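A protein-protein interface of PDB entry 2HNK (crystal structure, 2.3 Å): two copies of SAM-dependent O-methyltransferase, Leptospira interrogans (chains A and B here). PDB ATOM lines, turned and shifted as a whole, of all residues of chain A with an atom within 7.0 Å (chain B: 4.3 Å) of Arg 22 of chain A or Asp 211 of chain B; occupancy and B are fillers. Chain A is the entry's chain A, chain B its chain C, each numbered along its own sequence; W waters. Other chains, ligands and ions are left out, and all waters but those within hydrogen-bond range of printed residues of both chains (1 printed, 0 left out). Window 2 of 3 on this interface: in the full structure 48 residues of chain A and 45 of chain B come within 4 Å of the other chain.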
ATOM      1  N   PHE A  17      32.328  -9.265  15.279  1.00  0.00           N
ATOM      2  CA  PHE A  17      31.205  -9.223  16.213  1.00  0.00           C
ATOM      3  C   PHE A  17      31.433  -8.177  17.307  1.00  0.00           C
ATOM      4  O   PHE A  17      30.572  -7.331  17.550  1.00  0.00           O
ATOM      5  CB  PHE A  17      30.985 -10.613  16.829  1.00  0.00           C
ATOM      6  CG  PHE A  17      29.854 -10.673  17.812  1.00  0.00           C
ATOM      7  CD1 PHE A  17      28.535 -10.806  17.373  1.00  0.00           C
ATOM      8  CD2 PHE A  17      30.098 -10.594  19.178  1.00  0.00           C
ATOM      9  CE1 PHE A  17      27.489 -10.863  18.274  1.00  0.00           C
ATOM     10  CE2 PHE A  17      29.046 -10.652  20.093  1.00  0.00           C
ATOM     11  CZ  PHE A  17      27.743 -10.787  19.637  1.00  0.00           C
ATOM     12  N   ASN A  19      33.376  -5.660  17.396  1.00  0.00           N
ATOM     13  CA  ASN A  19      33.597  -4.309  16.886  1.00  0.00           C
ATOM     14  C   ASN A  19      32.502  -3.712  16.000  1.00  0.00           C
ATOM     15  O   ASN A  19      32.696  -2.643  15.424  1.00  0.00           O
ATOM     16  CB  ASN A  19      34.949  -4.232  16.179  1.00  0.00           C
ATOM     17  CG  ASN A  19      36.091  -4.220  17.149  1.00  0.00           C
ATOM     18  OD1 ASN A  19      36.534  -3.154  17.577  1.00  0.00           O
ATOM     19  ND2 ASN A  19      36.554  -5.402  17.542  1.00  0.00           N
ATOM     20  N   SER A  20      31.359  -4.385  15.902  1.00  0.00           N
ATOM     21  CA  SER A  20      30.246  -3.876  15.089  1.00  0.00           C
ATOM     22  C   SER A  20      28.859  -4.144  15.685  1.00  0.00           C
ATOM     23  O   SER A  20      27.982  -3.290  15.595  1.00  0.00           O
ATOM     24  CB  SER A  20      30.322  -4.396  13.642  1.00  0.00           C
ATOM     25  OG  SER A  20      30.197  -5.809  13.576  1.00  0.00           O
ATOM     26  N   VAL A  21      28.670  -5.312  16.302  1.00  0.00           N
ATOM     27  CA  VAL A  21      27.340  -5.745  16.734  1.00  0.00           C
ATOM     28  C   VAL A  21      26.941  -5.198  18.102  1.00  0.00           C
ATOM     29  O   VAL A  21      27.597  -5.468  19.109  1.00  0.00           O
ATOM     30  CB  VAL A  21      27.163  -7.300  16.665  1.00  0.00           C
ATOM     31  CG1 VAL A  21      25.869  -7.738  17.342  1.00  0.00           C
ATOM     32  CG2 VAL A  21      27.164  -7.776  15.219  1.00  0.00           C
ATOM     33  N   ARG A  22      25.865  -4.411  18.109  1.00  0.00           N
ATOM     34  CA  ARG A  22      25.273  -3.860  19.320  1.00  0.00           C
ATOM     35  C   ARG A  22      23.829  -4.374  19.359  1.00  0.00           C
ATOM     36  O   ARG A  22      22.894  -3.683  18.939  1.00  0.00           O
ATOM     37  CB  ARG A  22      25.292  -2.317  19.312  1.00  0.00           C
ATOM     38  CG  ARG A  22      26.525  -1.623  18.678  1.00  0.00           C
ATOM     39  CD  ARG A  22      26.393  -0.077  18.771  1.00  0.00           C
ATOM     40  NE  ARG A  22      27.443   0.684  18.077  1.00  0.00           N
ATOM     41  CZ  ARG A  22      27.366   1.995  17.805  1.00  0.00           C
ATOM     42  NH1 ARG A  22      26.289   2.696  18.163  1.00  0.00           N
ATOM     43  NH2 ARG A  22      28.358   2.620  17.167  1.00  0.00           N
ATOM     44  N   GLU A  23      23.653  -5.595  19.850  1.00  0.00           N
ATOM     45  CA  GLU A  23      22.380  -6.289  19.708  1.00  0.00           C
ATOM     46  C   GLU A  23      21.476  -6.119  20.919  1.00  0.00           C
ATOM     47  O   GLU A  23      21.882  -6.430  22.042  1.00  0.00           O
ATOM     48  CB  GLU A  23      22.613  -7.777  19.431  1.00  0.00           C
ATOM     49  CG  GLU A  23      21.381  -8.536  18.947  1.00  0.00           C
ATOM     50  CD  GLU A  23      21.646 -10.012  18.737  1.00  0.00           C
ATOM     51  OE1 GLU A  23      20.951 -10.630  17.903  1.00  0.00           O
ATOM     52  OE2 GLU A  23      22.556 -10.560  19.398  1.00  0.00           O
ATOM     53  N   PRO A  24      20.237  -5.643  20.696  1.00  0.00           N
ATOM     54  CA  PRO A  24      19.240  -5.594  21.766  1.00  0.00           C
ATOM     55  C   PRO A  24      18.963  -6.983  22.328  1.00  0.00           C
ATOM     56  O   PRO A  24      18.942  -7.962  21.573  1.00  0.00           O
ATOM     57  CB  PRO A  24      17.992  -5.049  21.061  1.00  0.00           C
ATOM     58  CG  PRO A  24      18.515  -4.307  19.876  1.00  0.00           C
ATOM     59  CD  PRO A  24      19.700  -5.117  19.424  1.00  0.00           C
ATOM     60  N   PHE A  27      16.423  -9.200  20.555  1.00  0.00           N
ATOM     61  CA  PHE A  27      16.910  -9.793  19.302  1.00  0.00           C
ATOM     62  C   PHE A  27      17.734 -11.047  19.596  1.00  0.00           C
ATOM     63  O   PHE A  27      17.592 -12.067  18.912  1.00  0.00           O
ATOM     64  CB  PHE A  27      17.788  -8.798  18.524  1.00  0.00           C
ATOM     65  CG  PHE A  27      17.044  -7.635  17.905  1.00  0.00           C
ATOM     66  CD1 PHE A  27      16.080  -6.919  18.616  1.00  0.00           C
ATOM     67  CD2 PHE A  27      17.362  -7.215  16.617  1.00  0.00           C
ATOM     68  CE1 PHE A  27      15.428  -5.823  18.037  1.00  0.00           C
ATOM     69  CE2 PHE A  27      16.711  -6.130  16.026  1.00  0.00           C
ATOM     70  CZ  PHE A  27      15.750  -5.428  16.736  1.00  0.00           C
ATOM     71  N   PRO A  46      23.478 -11.797  13.637  1.00  0.00           N
ATOM     72  CA  PRO A  46      23.270 -10.403  14.029  1.00  0.00           C
ATOM     73  C   PRO A  46      24.015  -9.412  13.120  1.00  0.00           C
ATOM     74  O   PRO A  46      23.545  -8.295  12.924  1.00  0.00           O
ATOM     75  CB  PRO A  46      23.800 -10.349  15.472  1.00  0.00           C
ATOM     76  CG  PRO A  46      24.626 -11.556  15.640  1.00  0.00           C
ATOM     77  CD  PRO A  46      24.062 -12.594  14.730  1.00  0.00           C
ATOM     78  N   GLN A  50      22.369  -6.155  11.138  1.00  0.00           N
ATOM     79  CA  GLN A  50      22.848  -4.771  11.230  1.00  0.00           C
ATOM     80  C   GLN A  50      23.191  -4.200   9.855  1.00  0.00           C
ATOM     81  O   GLN A  50      23.107  -2.991   9.628  1.00  0.00           O
ATOM     82  CB  GLN A  50      24.066  -4.675  12.158  1.00  0.00           C
ATOM     83  CG  GLN A  50      23.756  -4.988  13.617  1.00  0.00           C
ATOM     84  CD  GLN A  50      24.710  -4.317  14.600  1.00  0.00           C
ATOM     85  OE1 GLN A  50      24.493  -4.363  15.811  1.00  0.00           O
ATOM     86  NE2 GLN A  50      25.765  -3.687  14.082  1.00  0.00           N
ATOM     87  N   TYR B 164      38.772  10.411  11.520  1.00  0.00           N
ATOM     88  CA  TYR B 164      37.411  10.171  11.998  1.00  0.00           C
ATOM     89  C   TYR B 164      36.637  11.420  12.470  1.00  0.00           C
ATOM     90  O   TYR B 164      35.574  11.719  11.917  1.00  0.00           O
ATOM     91  CB  TYR B 164      37.400   9.049  13.042  1.00  0.00           C
ATOM     92  CG  TYR B 164      36.016   8.656  13.490  1.00  0.00           C
ATOM     93  CD1 TYR B 164      35.129   8.029  12.612  1.00  0.00           C
ATOM     94  CD2 TYR B 164      35.587   8.909  14.796  1.00  0.00           C
ATOM     95  CE1 TYR B 164      33.839   7.672  13.028  1.00  0.00           C
ATOM     96  CE2 TYR B 164      34.307   8.551  15.217  1.00  0.00           C
ATOM     97  CZ  TYR B 164      33.439   7.940  14.326  1.00  0.00           C
ATOM     98  OH  TYR B 164      32.176   7.581  14.737  1.00  0.00           O
ATOM     99  N   LEU B 168      33.399  13.187  10.494  1.00  0.00           N
ATOM    100  CA  LEU B 168      32.128  13.274  11.187  1.00  0.00           C
ATOM    101  C   LEU B 168      31.604  14.710  11.205  1.00  0.00           C
ATOM    102  O   LEU B 168      30.394  14.936  11.166  1.00  0.00           O
ATOM    103  CB  LEU B 168      32.307  12.756  12.611  1.00  0.00           C
ATOM    104  CG  LEU B 168      31.340  11.693  13.115  1.00  0.00           C
ATOM    105  CD1 LEU B 168      31.208  10.543  12.120  1.00  0.00           C
ATOM    106  CD2 LEU B 168      31.817  11.193  14.479  1.00  0.00           C
ATOM    107  N   LEU B 207      36.694   3.323  18.152  1.00  0.00           N
ATOM    108  CA  LEU B 207      36.000   4.621  18.184  1.00  0.00           C
ATOM    109  C   LEU B 207      34.600   4.542  17.573  1.00  0.00           C
ATOM    110  O   LEU B 207      33.627   5.031  18.151  1.00  0.00           O
ATOM    111  CB  LEU B 207      36.800   5.687  17.423  1.00  0.00           C
ATOM    112  CG  LEU B 207      37.928   6.448  18.118  1.00  0.00           C
ATOM    113  CD1 LEU B 207      38.747   7.239  17.090  1.00  0.00           C
ATOM    114  CD2 LEU B 207      37.369   7.374  19.215  1.00  0.00           C
ATOM    115  N   VAL B 208      34.523   3.933  16.392  1.00  0.00           N
ATOM    116  CA  VAL B 208      33.270   3.787  15.655  1.00  0.00           C
ATOM    117  C   VAL B 208      32.260   2.968  16.460  1.00  0.00           C
ATOM    118  O   VAL B 208      31.111   3.371  16.622  1.00  0.00           O
ATOM    119  CB  VAL B 208      33.529   3.130  14.277  1.00  0.00           C
ATOM    120  CG1 VAL B 208      32.235   2.649  13.650  1.00  0.00           C
ATOM    121  CG2 VAL B 208      34.281   4.086  13.356  1.00  0.00           C
ATOM    122  N   TYR B 209      32.719   1.827  16.974  1.00  0.00           N
ATOM    123  CA  TYR B 209      31.890   0.926  17.764  1.00  0.00           C
ATOM    124  C   TYR B 209      31.292   1.558  19.012  1.00  0.00           C
ATOM    125  O   TYR B 209      30.165   1.251  19.374  1.00  0.00           O
ATOM    126  CB  TYR B 209      32.677  -0.318  18.175  1.00  0.00           C
ATOM    127  CG  TYR B 209      31.835  -1.311  18.940  1.00  0.00           C
ATOM    128  CD1 TYR B 209      30.783  -1.979  18.318  1.00  0.00           C
ATOM    129  CD2 TYR B 209      32.079  -1.573  20.286  1.00  0.00           C
ATOM    130  CE1 TYR B 209      30.003  -2.885  19.008  1.00  0.00           C
ATOM    131  CE2 TYR B 209      31.299  -2.482  20.990  1.00  0.00           C
ATOM    132  CZ  TYR B 209      30.266  -3.132  20.340  1.00  0.00           C
ATOM    133  OH  TYR B 209      29.489  -4.037  21.016  1.00  0.00           O
ATOM    134  N   ASN B 210      32.051   2.421  19.675  1.00  0.00           N
ATOM    135  CA  ASN B 210      31.608   3.003  20.931  1.00  0.00           C
ATOM    136  C   ASN B 210      30.954   4.369  20.748  1.00  0.00           C
ATOM    137  O   ASN B 210      30.504   4.982  21.712  1.00  0.00           O
ATOM    138  CB  ASN B 210      32.781   3.071  21.912  1.00  0.00           C
ATOM    139  CG  ASN B 210      33.279   1.688  22.323  1.00  0.00           C
ATOM    140  OD1 ASN B 210      32.548   0.905  22.930  1.00  0.00           O
ATOM    141  ND2 ASN B 210      34.524   1.382  21.992  1.00  0.00           N
ATOM    142  N   ASP B 211      30.894   4.831  19.503  1.00  0.00           N
ATOM    143  CA  ASP B 211      30.298   6.120  19.170  1.00  0.00           C
ATOM    144  C   ASP B 211      28.786   6.003  18.961  1.00  0.00           C
ATOM    145  O   ASP B 211      28.327   5.359  18.011  1.00  0.00           O
ATOM    146  CB  ASP B 211      30.958   6.701  17.918  1.00  0.00           C
ATOM    147  CG  ASP B 211      30.680   8.176  17.742  1.00  0.00           C
ATOM    148  OD1 ASP B 211      29.867   8.724  18.509  1.00  0.00           O
ATOM    149  OD2 ASP B 211      31.271   8.787  16.828  1.00  0.00           O
ATOM    150  N   SER B 212      28.025   6.632  19.853  1.00  0.00           N
ATOM    151  CA  SER B 212      26.560   6.583  19.814  1.00  0.00           C
ATOM    152  C   SER B 212      26.001   7.515  18.748  1.00  0.00           C
ATOM    153  O   SER B 212      24.822   7.465  18.432  1.00  0.00           O
ATOM    154  CB  SER B 212      25.974   6.933  21.184  1.00  0.00           C
ATOM    155  OG  SER B 212      26.355   8.247  21.561  1.00  0.00           O
ATOM    156  N   LEU B 213      26.860   8.357  18.187  1.00  0.00           N
ATOM    157  CA  LEU B 213      26.460   9.270  17.124  1.00  0.00           C
ATOM    158  C   LEU B 213      26.396   8.593  15.754  1.00  0.00           C
ATOM    159  O   LEU B 213      25.930   9.201  14.785  1.00  0.00           O
ATOM    160  CB  LEU B 213      27.399  10.483  17.070  1.00  0.00           C
ATOM    161  CG  LEU B 213      27.434  11.447  18.269  1.00  0.00           C
ATOM    162  CD1 LEU B 213      28.249  12.669  17.898  1.00  0.00           C
ATOM    163  CD2 LEU B 213      26.044  11.868  18.711  1.00  0.00           C
ATOM    164  N   VAL B 214      26.866   7.348  15.676  1.00  0.00           N
ATOM    165  CA  VAL B 214      26.880   6.594  14.421  1.00  0.00           C
ATOM    166  C   VAL B 214      26.364   5.162  14.583  1.00  0.00           C
ATOM    167  O   VAL B 214      26.224   4.663  15.697  1.00  0.00           O
ATOM    168  CB  VAL B 214      28.309   6.544  13.768  1.00  0.00           C
ATOM    169  CG1 VAL B 214      28.936   7.938  13.682  1.00  0.00           C
ATOM    170  CG2 VAL B 214      29.237   5.568  14.515  1.00  0.00           C
ATOM    171  N   VAL B 216      27.226   1.217  12.710  1.00  0.00           N
ATOM    172  CA  VAL B 216      28.261   0.550  11.923  1.00  0.00           C
ATOM    173  C   VAL B 216      27.857  -0.846  11.431  1.00  0.00           C
ATOM    174  O   VAL B 216      27.258  -1.635  12.160  1.00  0.00           O
ATOM    175  CB  VAL B 216      29.637   0.514  12.688  1.00  0.00           C
ATOM    176  CG1 VAL B 216      29.489  -0.098  14.079  1.00  0.00           C
ATOM    177  CG2 VAL B 216      30.731  -0.198  11.874  1.00  0.00           C
HETATM  178  O   HOH W   1      29.221  -6.910  20.345  1.00  0.00           O
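The guanidinium group of Arg 22 of chain A lies within hydrogen-bond range of the backbone carbonyl oxygen of Val 214 of chain B (3.2 Å). The backbone carbonyl oxygen of Val 216 of chain B lies within hydrogen-bond range of the side-chain amide nitrogen of Gln 50 of chain A (3.2 Å). NE of Arg 22 of chain A lies within hydrogen-bond range of O of Tyr 209 of chain B (3.1 Å). The guanidinium group (NH2) of Arg 22 of chain A sits at hydrogen-bond distance from the backbone carbonyl oxygen (O) of Val 208 of chain B, 2.9 Å away. The side-chain hydroxyl of Tyr 209 of chain B is in hydrogen-bond range of the backbone carbonyl oxygen of Val 21 of chain A (3.0 Å). The guanidinium group (NH2) of Arg 22 of chain A lies within hydrogen-bond range of the backbone carbonyl oxygen (O) of Asp 211 of chain B.
The side-chain carboxylate of Asp 211 of chain B sits at hydrogen-bond distance from the backbone NH of Leu 213 of chain B. The backbone carbonyl oxygen of Ser 20 of chain A lies within hydrogen-bond range of the side-chain amide nitrogen of Gln 50 of chain A (2.7 Å). The side-chain hydroxyl (OH) of Tyr 164 of chain B sits at hydrogen-bond distance from the side-chain carboxylate (OD2) of Asp 211 of chain B. OE1 of Gln 50 of chain A sits at hydrogen-bond distance from N of Arg 22 of chain A (2.7 Å).
Among the printed residues, merely in contact across the chains: Asn 19 of chain A with Tyr 209 of chain B, Ser 20 of chain A with Tyr 209 of chain B and Ser 20 of chain A with Val 216 of chain B.
Of chain B, only Val 208 (2.9 Å), Tyr 209 (3.1 Å), Asp 211 (2.9 Å) and Val 214 (3.2 Å) come within 4 Å of Arg 22 of chain A. Of chain A, only Arg 22 comes within 4 Å of Asp 211 of chain B. Printed residues of chain A within 4 Å of Val 208 of chain B: Arg 22. Printed residues of chain A within 4 Å of Val 214 of chain B: Arg 22 (3.2 Å). The nearest residue of chain B that does not touch Arg 22 of chain A is Ser 212 of chain B (4.2 Å). The nearest printed residue of chain A that does not touch Asp 211 of chain B is Asn 19 of chain A (8.7 Å).
Of the 10 printed residues of chain A, 5 touch a printed residue of chain B.
No position is printed for both chains. Of the 9 pairs that touch across the chains among the printed residues, none has its exchanged pair printed and touching as well.
Water W1 lies within hydrogen-bond range of O of Val 21 of chain A, OH of Tyr 209 of chain B and O of Phe 17 of chain A.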
